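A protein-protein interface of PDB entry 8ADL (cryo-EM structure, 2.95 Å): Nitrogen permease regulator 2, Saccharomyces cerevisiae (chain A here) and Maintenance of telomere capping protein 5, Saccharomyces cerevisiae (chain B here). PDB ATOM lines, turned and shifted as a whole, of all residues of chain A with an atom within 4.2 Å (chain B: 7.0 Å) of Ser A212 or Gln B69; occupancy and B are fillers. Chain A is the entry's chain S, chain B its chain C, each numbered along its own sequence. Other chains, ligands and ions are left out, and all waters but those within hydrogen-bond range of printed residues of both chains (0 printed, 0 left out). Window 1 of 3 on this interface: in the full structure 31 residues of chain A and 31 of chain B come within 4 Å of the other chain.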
ATOM      1  N   PHE A   8     -16.421 -13.239 -24.190  1.00  0.00           N
ATOM      2  CA  PHE A   8     -17.435 -13.384 -23.157  1.00  0.00           C
ATOM      3  C   PHE A   8     -17.399 -12.181 -22.225  1.00  0.00           C
ATOM      4  O   PHE A   8     -16.324 -11.732 -21.814  1.00  0.00           O
ATOM      5  CB  PHE A   8     -17.217 -14.675 -22.366  1.00  0.00           C
ATOM      6  CG  PHE A   8     -17.337 -15.918 -23.198  1.00  0.00           C
ATOM      7  CD1 PHE A   8     -18.274 -15.998 -24.219  1.00  0.00           C
ATOM      8  CD2 PHE A   8     -16.492 -16.995 -22.985  1.00  0.00           C
ATOM      9  CE1 PHE A   8     -18.382 -17.140 -24.991  1.00  0.00           C
ATOM     10  CE2 PHE A   8     -16.590 -18.134 -23.757  1.00  0.00           C
ATOM     11  CZ  PHE A   8     -17.538 -18.209 -24.761  1.00  0.00           C
ATOM     12  N   ASP A 207     -13.589 -16.979 -11.289  1.00  0.00           N
ATOM     13  CA  ASP A 207     -13.294 -18.041 -12.240  1.00  0.00           C
ATOM     14  C   ASP A 207     -13.970 -17.786 -13.581  1.00  0.00           C
ATOM     15  O   ASP A 207     -13.398 -18.090 -14.634  1.00  0.00           O
ATOM     16  CB  ASP A 207     -13.710 -19.392 -11.659  1.00  0.00           C
ATOM     17  CG  ASP A 207     -12.771 -19.872 -10.567  1.00  0.00           C
ATOM     18  OD1 ASP A 207     -11.727 -19.225 -10.348  1.00  0.00           O
ATOM     19  OD2 ASP A 207     -13.081 -20.898  -9.924  1.00  0.00           O
ATOM     20  N   LEU A 208     -15.187 -17.229 -13.571  1.00  0.00           N
ATOM     21  CA  LEU A 208     -15.837 -16.889 -14.828  1.00  0.00           C
ATOM     22  C   LEU A 208     -15.311 -15.593 -15.432  1.00  0.00           C
ATOM     23  O   LEU A 208     -15.453 -15.393 -16.643  1.00  0.00           O
ATOM     24  CB  LEU A 208     -17.351 -16.791 -14.629  1.00  0.00           C
ATOM     25  CG  LEU A 208     -18.095 -18.105 -14.379  1.00  0.00           C
ATOM     26  CD1 LEU A 208     -19.597 -17.874 -14.350  1.00  0.00           C
ATOM     27  CD2 LEU A 208     -17.732 -19.143 -15.433  1.00  0.00           C
ATOM     28  N   ASN A 209     -14.710 -14.711 -14.630  1.00  0.00           N
ATOM     29  CA  ASN A 209     -14.109 -13.500 -15.171  1.00  0.00           C
ATOM     30  C   ASN A 209     -12.650 -13.674 -15.573  1.00  0.00           C
ATOM     31  O   ASN A 209     -12.115 -12.809 -16.277  1.00  0.00           O
ATOM     32  CB  ASN A 209     -14.219 -12.356 -14.157  1.00  0.00           C
ATOM     33  CG  ASN A 209     -15.630 -11.811 -14.043  1.00  0.00           C
ATOM     34  OD1 ASN A 209     -16.597 -12.479 -14.410  1.00  0.00           O
ATOM     35  ND2 ASN A 209     -15.752 -10.590 -13.535  1.00  0.00           N
ATOM     36  N   ASN A 210     -11.994 -14.756 -15.155  1.00  0.00           N
ATOM     37  CA  ASN A 210     -10.584 -14.958 -15.462  1.00  0.00           C
ATOM     38  C   ASN A 210     -10.307 -16.166 -16.340  1.00  0.00           C
ATOM     39  O   ASN A 210      -9.285 -16.184 -17.030  1.00  0.00           O
ATOM     40  CB  ASN A 210      -9.766 -15.094 -14.167  1.00  0.00           C
ATOM     41  CG  ASN A 210      -9.470 -13.756 -13.519  1.00  0.00           C
ATOM     42  OD1 ASN A 210      -9.193 -12.771 -14.201  1.00  0.00           O
ATOM     43  ND2 ASN A 210      -9.529 -13.714 -12.194  1.00  0.00           N
ATOM     44  N   TYR A 211     -11.178 -17.175 -16.334  1.00  0.00           N
ATOM     45  CA  TYR A 211     -10.924 -18.410 -17.062  1.00  0.00           C
ATOM     46  C   TYR A 211     -12.068 -18.845 -17.964  1.00  0.00           C
ATOM     47  O   TYR A 211     -11.865 -19.758 -18.774  1.00  0.00           O
ATOM     48  CB  TYR A 211     -10.604 -19.550 -16.081  1.00  0.00           C
ATOM     49  CG  TYR A 211      -9.593 -19.169 -15.024  1.00  0.00           C
ATOM     50  CD1 TYR A 211      -8.241 -19.089 -15.329  1.00  0.00           C
ATOM     51  CD2 TYR A 211      -9.991 -18.874 -13.724  1.00  0.00           C
ATOM     52  CE1 TYR A 211      -7.310 -18.731 -14.370  1.00  0.00           C
ATOM     53  CE2 TYR A 211      -9.066 -18.518 -12.757  1.00  0.00           C
ATOM     54  CZ  TYR A 211      -7.728 -18.447 -13.088  1.00  0.00           C
ATOM     55  OH  TYR A 211      -6.801 -18.098 -12.134  1.00  0.00           O
ATOM     56  N   SER A 212     -13.255 -18.236 -17.838  1.00  0.00           N
ATOM     57  CA  SER A 212     -14.503 -18.683 -18.476  1.00  0.00           C
ATOM     58  C   SER A 212     -14.846 -20.135 -18.137  1.00  0.00           C
ATOM     59  O   SER A 212     -15.522 -20.817 -18.909  1.00  0.00           O
ATOM     60  CB  SER A 212     -14.473 -18.476 -19.996  1.00  0.00           C
ATOM     61  OG  SER A 212     -14.711 -17.118 -20.323  1.00  0.00           O
ATOM     62  N   GLU A 213     -14.410 -20.597 -16.965  1.00  0.00           N
ATOM     63  CA  GLU A 213     -14.586 -21.972 -16.519  1.00  0.00           C
ATOM     64  C   GLU A 213     -14.487 -21.982 -15.002  1.00  0.00           C
ATOM     65  O   GLU A 213     -13.869 -21.099 -14.406  1.00  0.00           O
ATOM     66  CB  GLU A 213     -13.530 -22.912 -17.115  1.00  0.00           C
ATOM     67  CG  GLU A 213     -13.896 -23.557 -18.439  1.00  0.00           C
ATOM     68  CD  GLU A 213     -12.847 -24.545 -18.892  1.00  0.00           C
ATOM     69  OE1 GLU A 213     -12.058 -24.993 -18.036  1.00  0.00           O
ATOM     70  OE2 GLU A 213     -12.801 -24.866 -20.097  1.00  0.00           O
ATOM     71  N   LYS A 227     -18.890 -24.133 -17.823  1.00  0.00           N
ATOM     72  CA  LYS A 227     -18.050 -23.711 -18.937  1.00  0.00           C
ATOM     73  C   LYS A 227     -18.886 -22.885 -19.902  1.00  0.00           C
ATOM     74  O   LYS A 227     -19.958 -23.324 -20.331  1.00  0.00           O
ATOM     75  CB  LYS A 227     -17.431 -24.905 -19.661  1.00  0.00           C
ATOM     76  CG  LYS A 227     -16.835 -24.575 -21.017  1.00  0.00           C
ATOM     77  CD  LYS A 227     -15.782 -25.595 -21.409  1.00  0.00           C
ATOM     78  CE  LYS A 227     -14.974 -25.128 -22.606  1.00  0.00           C
ATOM     79  NZ  LYS A 227     -13.730 -25.929 -22.776  1.00  0.00           N
ATOM     80  N   ILE A 228     -18.398 -21.697 -20.239  1.00  0.00           N
ATOM     81  CA  ILE A 228     -19.114 -20.774 -21.111  1.00  0.00           C
ATOM     82  C   ILE A 228     -18.722 -21.065 -22.555  1.00  0.00           C
ATOM     83  O   ILE A 228     -17.541 -20.995 -22.913  1.00  0.00           O
ATOM     84  CB  ILE A 228     -18.813 -19.316 -20.738  1.00  0.00           C
ATOM     85  CG1 ILE A 228     -19.161 -19.066 -19.270  1.00  0.00           C
ATOM     86  CG2 ILE A 228     -19.587 -18.370 -21.631  1.00  0.00           C
ATOM     87  CD1 ILE A 228     -20.624 -19.266 -18.952  1.00  0.00           C
ATOM     88  N   GLY B  25      -7.929  -3.434 -25.055  1.00  0.00           N
ATOM     89  CA  GLY B  25      -8.131  -4.738 -25.656  1.00  0.00           C
ATOM     90  C   GLY B  25      -8.547  -5.812 -24.672  1.00  0.00           C
ATOM     91  O   GLY B  25      -8.948  -6.908 -25.075  1.00  0.00           O
ATOM     92  N   GLY B  26      -8.467  -5.509 -23.379  1.00  0.00           N
ATOM     93  CA  GLY B  26      -8.845  -6.470 -22.362  1.00  0.00           C
ATOM     94  C   GLY B  26      -7.838  -7.587 -22.192  1.00  0.00           C
ATOM     95  O   GLY B  26      -8.143  -8.753 -22.461  1.00  0.00           O
ATOM     96  N   PHE B  27      -6.634  -7.247 -21.737  1.00  0.00           N
ATOM     97  CA  PHE B  27      -5.569  -8.224 -21.550  1.00  0.00           C
ATOM     98  C   PHE B  27      -5.599  -8.760 -20.124  1.00  0.00           C
ATOM     99  O   PHE B  27      -5.672  -7.988 -19.163  1.00  0.00           O
ATOM    100  CB  PHE B  27      -4.210  -7.593 -21.858  1.00  0.00           C
ATOM    101  CG  PHE B  27      -4.035  -7.210 -23.301  1.00  0.00           C
ATOM    102  CD1 PHE B  27      -4.452  -5.971 -23.760  1.00  0.00           C
ATOM    103  CD2 PHE B  27      -3.440  -8.085 -24.194  1.00  0.00           C
ATOM    104  CE1 PHE B  27      -4.297  -5.620 -25.087  1.00  0.00           C
ATOM    105  CE2 PHE B  27      -3.278  -7.739 -25.522  1.00  0.00           C
ATOM    106  CZ  PHE B  27      -3.707  -6.505 -25.968  1.00  0.00           C
ATOM    107  N   ASN B  28      -5.539 -10.087 -19.995  1.00  0.00           N
ATOM    108  CA  ASN B  28      -5.689 -10.743 -18.703  1.00  0.00           C
ATOM    109  C   ASN B  28      -4.383 -11.263 -18.116  1.00  0.00           C
ATOM    110  O   ASN B  28      -4.331 -11.522 -16.908  1.00  0.00           O
ATOM    111  CB  ASN B  28      -6.685 -11.906 -18.815  1.00  0.00           C
ATOM    112  CG  ASN B  28      -7.336 -12.247 -17.487  1.00  0.00           C
ATOM    113  OD1 ASN B  28      -7.764 -11.362 -16.746  1.00  0.00           O
ATOM    114  ND2 ASN B  28      -7.413 -13.536 -17.181  1.00  0.00           N
ATOM    115  N   ALA B  29      -3.331 -11.418 -18.919  1.00  0.00           N
ATOM    116  CA  ALA B  29      -2.085 -12.003 -18.445  1.00  0.00           C
ATOM    117  C   ALA B  29      -0.902 -11.145 -18.866  1.00  0.00           C
ATOM    118  O   ALA B  29      -0.956 -10.433 -19.873  1.00  0.00           O
ATOM    119  CB  ALA B  29      -1.900 -13.431 -18.973  1.00  0.00           C
ATOM    120  N   ALA B  42      -1.350 -10.775 -22.777  1.00  0.00           N
ATOM    121  CA  ALA B  42      -2.168 -11.811 -23.396  1.00  0.00           C
ATOM    122  C   ALA B  42      -3.646 -11.476 -23.245  1.00  0.00           C
ATOM    123  O   ALA B  42      -4.098 -11.120 -22.153  1.00  0.00           O
ATOM    124  CB  ALA B  42      -1.875 -13.180 -22.778  1.00  0.00           C
ATOM    125  N   SER B  43      -4.394 -11.605 -24.340  1.00  0.00           N
ATOM    126  CA  SER B  43      -5.843 -11.433 -24.335  1.00  0.00           C
ATOM    127  C   SER B  43      -6.455 -12.561 -25.155  1.00  0.00           C
ATOM    128  O   SER B  43      -5.764 -13.485 -25.592  1.00  0.00           O
ATOM    129  CB  SER B  43      -6.251 -10.058 -24.880  1.00  0.00           C
ATOM    130  OG  SER B  43      -5.773  -9.871 -26.200  1.00  0.00           O
ATOM    131  N   ARG B  44      -7.771 -12.481 -25.365  1.00  0.00           N
ATOM    132  CA  ARG B  44      -8.456 -13.459 -26.201  1.00  0.00           C
ATOM    133  C   ARG B  44      -8.101 -13.318 -27.675  1.00  0.00           C
ATOM    134  O   ARG B  44      -8.268 -14.280 -28.433  1.00  0.00           O
ATOM    135  CB  ARG B  44      -9.970 -13.331 -26.027  1.00  0.00           C
ATOM    136  CG  ARG B  44     -10.482 -13.737 -24.657  1.00  0.00           C
ATOM    137  CD  ARG B  44     -11.951 -13.379 -24.492  1.00  0.00           C
ATOM    138  NE  ARG B  44     -12.131 -12.047 -23.927  1.00  0.00           N
ATOM    139  CZ  ARG B  44     -12.992 -11.753 -22.963  1.00  0.00           C
ATOM    140  NH1 ARG B  44     -13.775 -12.676 -22.429  1.00  0.00           N
ATOM    141  NH2 ARG B  44     -13.073 -10.499 -22.526  1.00  0.00           N
ATOM    142  N   THR B  66      -9.525 -16.758 -29.650  1.00  0.00           N
ATOM    143  CA  THR B  66     -10.219 -17.738 -28.831  1.00  0.00           C
ATOM    144  C   THR B  66     -11.385 -17.059 -28.123  1.00  0.00           C
ATOM    145  O   THR B  66     -11.315 -15.861 -27.820  1.00  0.00           O
ATOM    146  CB  THR B  66      -9.263 -18.401 -27.818  1.00  0.00           C
ATOM    147  OG1 THR B  66      -9.940 -19.448 -27.109  1.00  0.00           O
ATOM    148  CG2 THR B  66      -8.667 -17.391 -26.841  1.00  0.00           C
ATOM    149  N   PRO B  67     -12.493 -17.782 -27.894  1.00  0.00           N
ATOM    150  CA  PRO B  67     -13.615 -17.173 -27.165  1.00  0.00           C
ATOM    151  C   PRO B  67     -13.417 -17.160 -25.658  1.00  0.00           C
ATOM    152  O   PRO B  67     -13.990 -16.315 -24.963  1.00  0.00           O
ATOM    153  CB  PRO B  67     -14.810 -18.049 -27.562  1.00  0.00           C
ATOM    154  CG  PRO B  67     -14.218 -19.354 -27.933  1.00  0.00           C
ATOM    155  CD  PRO B  67     -12.861 -19.069 -28.509  1.00  0.00           C
ATOM    156  N   TRP B  68     -12.613 -18.084 -25.138  1.00  0.00           N
ATOM    157  CA  TRP B  68     -12.387 -18.180 -23.704  1.00  0.00           C
ATOM    158  C   TRP B  68     -11.255 -17.255 -23.276  1.00  0.00           C
ATOM    159  O   TRP B  68     -10.329 -16.977 -24.042  1.00  0.00           O
ATOM    160  CB  TRP B  68     -12.073 -19.620 -23.296  1.00  0.00           C
ATOM    161  CG  TRP B  68     -13.169 -20.581 -23.630  1.00  0.00           C
ATOM    162  CD1 TRP B  68     -14.299 -20.817 -22.906  1.00  0.00           C
ATOM    163  CD2 TRP B  68     -13.236 -21.447 -24.771  1.00  0.00           C
ATOM    164  NE1 TRP B  68     -15.071 -21.770 -23.526  1.00  0.00           N
ATOM    165  CE2 TRP B  68     -14.439 -22.173 -24.673  1.00  0.00           C
ATOM    166  CE3 TRP B  68     -12.396 -21.677 -25.865  1.00  0.00           C
ATOM    167  CZ2 TRP B  68     -14.825 -23.113 -25.629  1.00  0.00           C
ATOM    168  CZ3 TRP B  68     -12.781 -22.609 -26.813  1.00  0.00           C
ATOM    169  CH2 TRP B  68     -13.984 -23.316 -26.688  1.00  0.00           C
ATOM    170  N   GLN B  69     -11.339 -16.778 -22.036  1.00  0.00           N
ATOM    171  CA  GLN B  69     -10.350 -15.844 -21.517  1.00  0.00           C
ATOM    172  C   GLN B  69      -9.034 -16.564 -21.242  1.00  0.00           C
ATOM    173  O   GLN B  69      -9.023 -17.654 -20.661  1.00  0.00           O
ATOM    174  CB  GLN B  69     -10.870 -15.181 -20.242  1.00  0.00           C
ATOM    175  CG  GLN B  69      -9.935 -14.141 -19.642  1.00  0.00           C
ATOM    176  CD  GLN B  69     -10.022 -12.803 -20.347  1.00  0.00           C
ATOM    177  OE1 GLN B  69      -9.255 -12.521 -21.268  1.00  0.00           O
ATOM    178  NE2 GLN B  69     -10.961 -11.969 -19.917  1.00  0.00           N
ATOM    179  N   VAL B  70      -7.923 -15.956 -21.665  1.00  0.00           N
ATOM    180  CA  VAL B  70      -6.614 -16.537 -21.397  1.00  0.00           C
ATOM    181  C   VAL B  70      -6.272 -16.361 -19.922  1.00  0.00           C
ATOM    182  O   VAL B  70      -6.706 -15.405 -19.263  1.00  0.00           O
ATOM    183  CB  VAL B  70      -5.532 -15.919 -22.302  1.00  0.00           C
ATOM    184  CG1 VAL B  70      -5.802 -16.263 -23.757  1.00  0.00           C
ATOM    185  CG2 VAL B  70      -5.462 -14.414 -22.110  1.00  0.00           C
ATOM    186  N   ALA B  71      -5.496 -17.306 -19.388  1.00  0.00           N
ATOM    187  CA  ALA B  71      -5.183 -17.325 -17.964  1.00  0.00           C
ATOM    188  C   ALA B  71      -3.792 -16.778 -17.657  1.00  0.00           C
ATOM    189  O   ALA B  71      -3.659 -15.813 -16.899  1.00  0.00           O
ATOM    190  CB  ALA B  71      -5.318 -18.752 -17.423  1.00  0.00           C
ATOM    191  N   ASP B  72      -2.750 -17.377 -18.231  1.00  0.00           N
ATOM    192  CA  ASP B  72      -1.391 -17.005 -17.871  1.00  0.00           C
ATOM    193  C   ASP B  72      -0.477 -17.019 -19.086  1.00  0.00           C
ATOM    194  O   ASP B  72      -0.697 -17.756 -20.050  1.00  0.00           O
ATOM    195  CB  ASP B  72      -0.822 -17.942 -16.798  1.00  0.00           C
ATOM    196  CG  ASP B  72       0.124 -17.233 -15.849  1.00  0.00           C
ATOM    197  OD1 ASP B  72      -0.099 -16.037 -15.569  1.00  0.00           O
ATOM    198  OD2 ASP B  72       1.093 -17.871 -15.387  1.00  0.00           O
ATOM    199  N   THR B  88      -1.447 -19.818 -22.401  1.00  0.00           N
ATOM    200  CA  THR B  88      -2.576 -20.732 -22.294  1.00  0.00           C
ATOM    201  C   THR B  88      -3.632 -20.352 -23.323  1.00  0.00           C
ATOM    202  O   THR B  88      -4.019 -19.183 -23.421  1.00  0.00           O
ATOM    203  CB  THR B  88      -3.173 -20.706 -20.887  1.00  0.00           C
ATOM    204  OG1 THR B  88      -3.777 -19.427 -20.644  1.00  0.00           O
ATOM    205  CG2 THR B  88      -2.096 -20.961 -19.843  1.00  0.00           C
ATOM    206  N   SER B  89      -4.094 -21.337 -24.086  1.00  0.00           N
ATOM    207  CA  SER B  89      -5.205 -21.166 -25.019  1.00  0.00           C
ATOM    208  C   SER B  89      -6.257 -22.208 -24.658  1.00  0.00           C
ATOM    209  O   SER B  89      -6.291 -23.289 -25.254  1.00  0.00           O
ATOM    210  CB  SER B  89      -4.749 -21.303 -26.464  1.00  0.00           C
ATOM    211  OG  SER B  89      -5.860 -21.374 -27.339  1.00  0.00           O
ATOM    212  N   ASN B  90      -7.114 -21.854 -23.695  1.00  0.00           N
ATOM    213  CA  ASN B  90      -8.089 -22.745 -23.069  1.00  0.00           C
ATOM    214  C   ASN B  90      -7.418 -24.013 -22.551  1.00  0.00           C
ATOM    215  O   ASN B  90      -6.602 -23.945 -21.627  1.00  0.00           O
ATOM    216  CB  ASN B  90      -9.227 -23.075 -24.039  1.00  0.00           C
ATOM    217  CG  ASN B  90     -10.498 -23.494 -23.328  1.00  0.00           C
ATOM    218  OD1 ASN B  90     -10.717 -23.152 -22.166  1.00  0.00           O
ATOM    219  ND2 ASN B  90     -11.342 -24.246 -24.024  1.00  0.00           N
ATOM    220  N   ARG B 115      -9.806 -29.410 -19.562  1.00  0.00           N
ATOM    221  CA  ARG B 115     -10.347 -28.094 -19.266  1.00  0.00           C
ATOM    222  C   ARG B 115      -9.226 -27.056 -19.289  1.00  0.00           C
ATOM    223  O   ARG B 115      -8.064 -27.368 -19.563  1.00  0.00           O
ATOM    224  CB  ARG B 115     -11.075 -28.107 -17.920  1.00  0.00           C
ATOM    225  CG  ARG B 115     -12.320 -28.978 -17.909  1.00  0.00           C
ATOM    226  CD  ARG B 115     -13.522 -28.243 -18.475  1.00  0.00           C
ATOM    227  NE  ARG B 115     -14.024 -27.224 -17.562  1.00  0.00           N
ATOM    228  CZ  ARG B 115     -14.885 -27.455 -16.580  1.00  0.00           C
ATOM    229  NH1 ARG B 115     -15.363 -28.667 -16.350  1.00  0.00           N
ATOM    230  NH2 ARG B 115     -15.274 -26.445 -15.807  1.00  0.00           N
ATOM    231  N   ALA B 116      -9.593 -25.804 -19.014  1.00  0.00           N
ATOM    232  CA  ALA B 116      -8.690 -24.676 -19.222  1.00  0.00           C
ATOM    233  C   ALA B 116      -7.506 -24.706 -18.261  1.00  0.00           C
ATOM    234  O   ALA B 116      -7.664 -24.936 -17.060  1.00  0.00           O
ATOM    235  CB  ALA B 116      -9.441 -23.353 -19.070  1.00  0.00           C
ATOM    236  N   ILE B 117      -6.316 -24.449 -18.807  1.00  0.00           N
ATOM    237  CA  ILE B 117      -5.099 -24.374 -18.006  1.00  0.00           C
ATOM    238  C   ILE B 117      -5.142 -23.118 -17.147  1.00  0.00           C
ATOM    239  O   ILE B 117      -5.372 -22.011 -17.651  1.00  0.00           O
ATOM    240  CB  ILE B 117      -3.859 -24.394 -18.913  1.00  0.00           C
ATOM    241  CG1 ILE B 117      -3.826 -25.684 -19.737  1.00  0.00           C
ATOM    242  CG2 ILE B 117      -2.587 -24.250 -18.086  1.00  0.00           C
ATOM    243  CD1 ILE B 117      -2.550 -25.881 -20.533  1.00  0.00           C
ATOM    244  N   LYS B 331      -7.109  -3.818 -14.504  1.00  0.00           N
ATOM    245  CA  LYS B 331      -8.312  -4.036 -15.297  1.00  0.00           C
ATOM    246  C   LYS B 331      -8.756  -2.790 -16.059  1.00  0.00           C
ATOM    247  O   LYS B 331      -9.494  -2.909 -17.044  1.00  0.00           O
ATOM    248  CB  LYS B 331      -9.441  -4.527 -14.383  1.00  0.00           C
ATOM    249  CG  LYS B 331     -10.631  -5.165 -15.091  1.00  0.00           C
ATOM    250  CD  LYS B 331     -10.234  -6.417 -15.854  1.00  0.00           C
ATOM    251  CE  LYS B 331     -10.000  -7.586 -14.911  1.00  0.00           C
ATOM    252  NZ  LYS B 331     -11.273  -8.062 -14.297  1.00  0.00           N
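Among the printed residues, merely in contact across the chains: Phe A8 with Pro B67 (3.3 Å), Phe A8 with Trp B68 (3.6 Å), Asn A209 with Gln B69 (3.9 Å), Asn A210 with Gln B69 (3.4 Å), Tyr A211 with Ala B71 (3.6 Å), Ser A212 with Trp B68 (3.7 Å), Ser A212 with Gln B69 (3.8 Å) and Lys A227 with Trp B68 (3.5 Å).
Printed residues of chain B that touch a printed residue of chain A: Asn B28, Arg B44, Pro B67, Trp B68, Gln B69, Val B70, Ala B71, Asn B90, Arg B115 and Ala B116.
Hydrophobic or aromatic side chains of chain B that line the printed part of chain A: Pro B67, Trp B68, Ala B71 and Ala B116.
Along chain B the printed residues that touch a printed residue of chain A span positions 28 to 116.
Of the 10 printed residues of chain A, 8 touch a printed residue of chain B.
Hydrophobic or aromatic side chains of chain A within 4 Å of the printed part of chain B: Phe A8 and Tyr A211.
Among the printed residues, Asp or Glu carboxylates within 4 Å of a Lys or Arg side-chain nitrogen of the other chain: Glu A213 with Arg B115.
O of Ser A212 lies within hydrogen-bond range of N of Ile A228 (3.3 Å).
The backbone NH (N) of Asn B28 sits at hydrogen-bond distance from the backbone carbonyl oxygen (O) of Ala B42.
The backbone NH (N) of Ala B71 sits at hydrogen-bond distance from the side-chain hydroxyl (OG1) of Thr B88 (3.0 Å).
The backbone carbonyl oxygen (O) of Val B70 is in hydrogen-bond range of the side-chain amide nitrogen (ND2) of Asn B28, 2.9 Å away.
The side-chain carboxylate (OE2) of Glu A213 lies within salt-bridge range of the side-chain amino group (NZ) of Lys A227, 3.0 Å away.
The backbone carbonyl oxygen (O) of Asp A207 sits at hydrogen-bond distance from the backbone NH (N) of Ser A212, 3.2 Å away.
The side-chain amide nitrogen (ND2) of Asn B90 lies close to the side-chain amino group (NZ) of Lys A227, at 3.2 Å.
OD1 of Asn A210 sits close to OD1 of Asn B28 (3.2 Å).
The backbone carbonyl oxygen (O) of Val B70 lies close to the backbone carbonyl oxygen (O) of Asn A210 (3.5 Å).
The indole nitrogen (NE1) of Trp B68 is in hydrogen-bond range of the backbone carbonyl oxygen (O) of Ile A228 (2.7 Å).
The side-chain carboxylate (OE1) of Glu A213 lies within hydrogen-bond range of the backbone NH (N) of Ala B116 (2.8 Å).
O of Phe A8 sits at hydrogen-bond distance from NH1 of Arg B44, 2.8 Å away.
NE of Arg B115 lies within salt-bridge range of OE1 of Glu A213 (3.0 Å).
OD1 of Asn B90 lies close to OE2 of Glu A213 (3.4 Å).
Ser A212 touches just these residues of chain B: Trp B68 (3.7 Å) and Gln B69 (3.8 Å).
Of the printed residues of chain A, Gln B69 touches Asn A209 (3.9 Å), Asn A210 (3.4 Å) and Ser A212 (3.8 Å).
Printed residues of chain B within 4 Å of Asn A209: Gln B69.
Of the printed residues of chain A, Arg B44 touches Phe A8.
Of the printed residues of chain A, Arg B115 touches Glu A213 (3.0 Å).
Of the printed residues of chain B, Ile A228 touches Trp B68 (2.7 Å).
Of the printed residues of chain A, Trp B68 touches Phe A8 (3.6 Å), Ser A212 (3.7 Å), Lys A227 (3.5 Å) and Ile A228 (2.7 Å).
Asp A207 touches none of the printed residues of chain B.
Lys B331 touches none of the printed residues of chain A.
The nearest residue of chain B that does not touch Ser A212 is Pro B67 (4.8 Å).
The nearest printed residue of chain A that does not touch Gln B69 is Tyr A211 (4.01 Å).
The nearest printed residue of chain B that does not touch Glu A213 is Trp B68 (5.1 Å).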
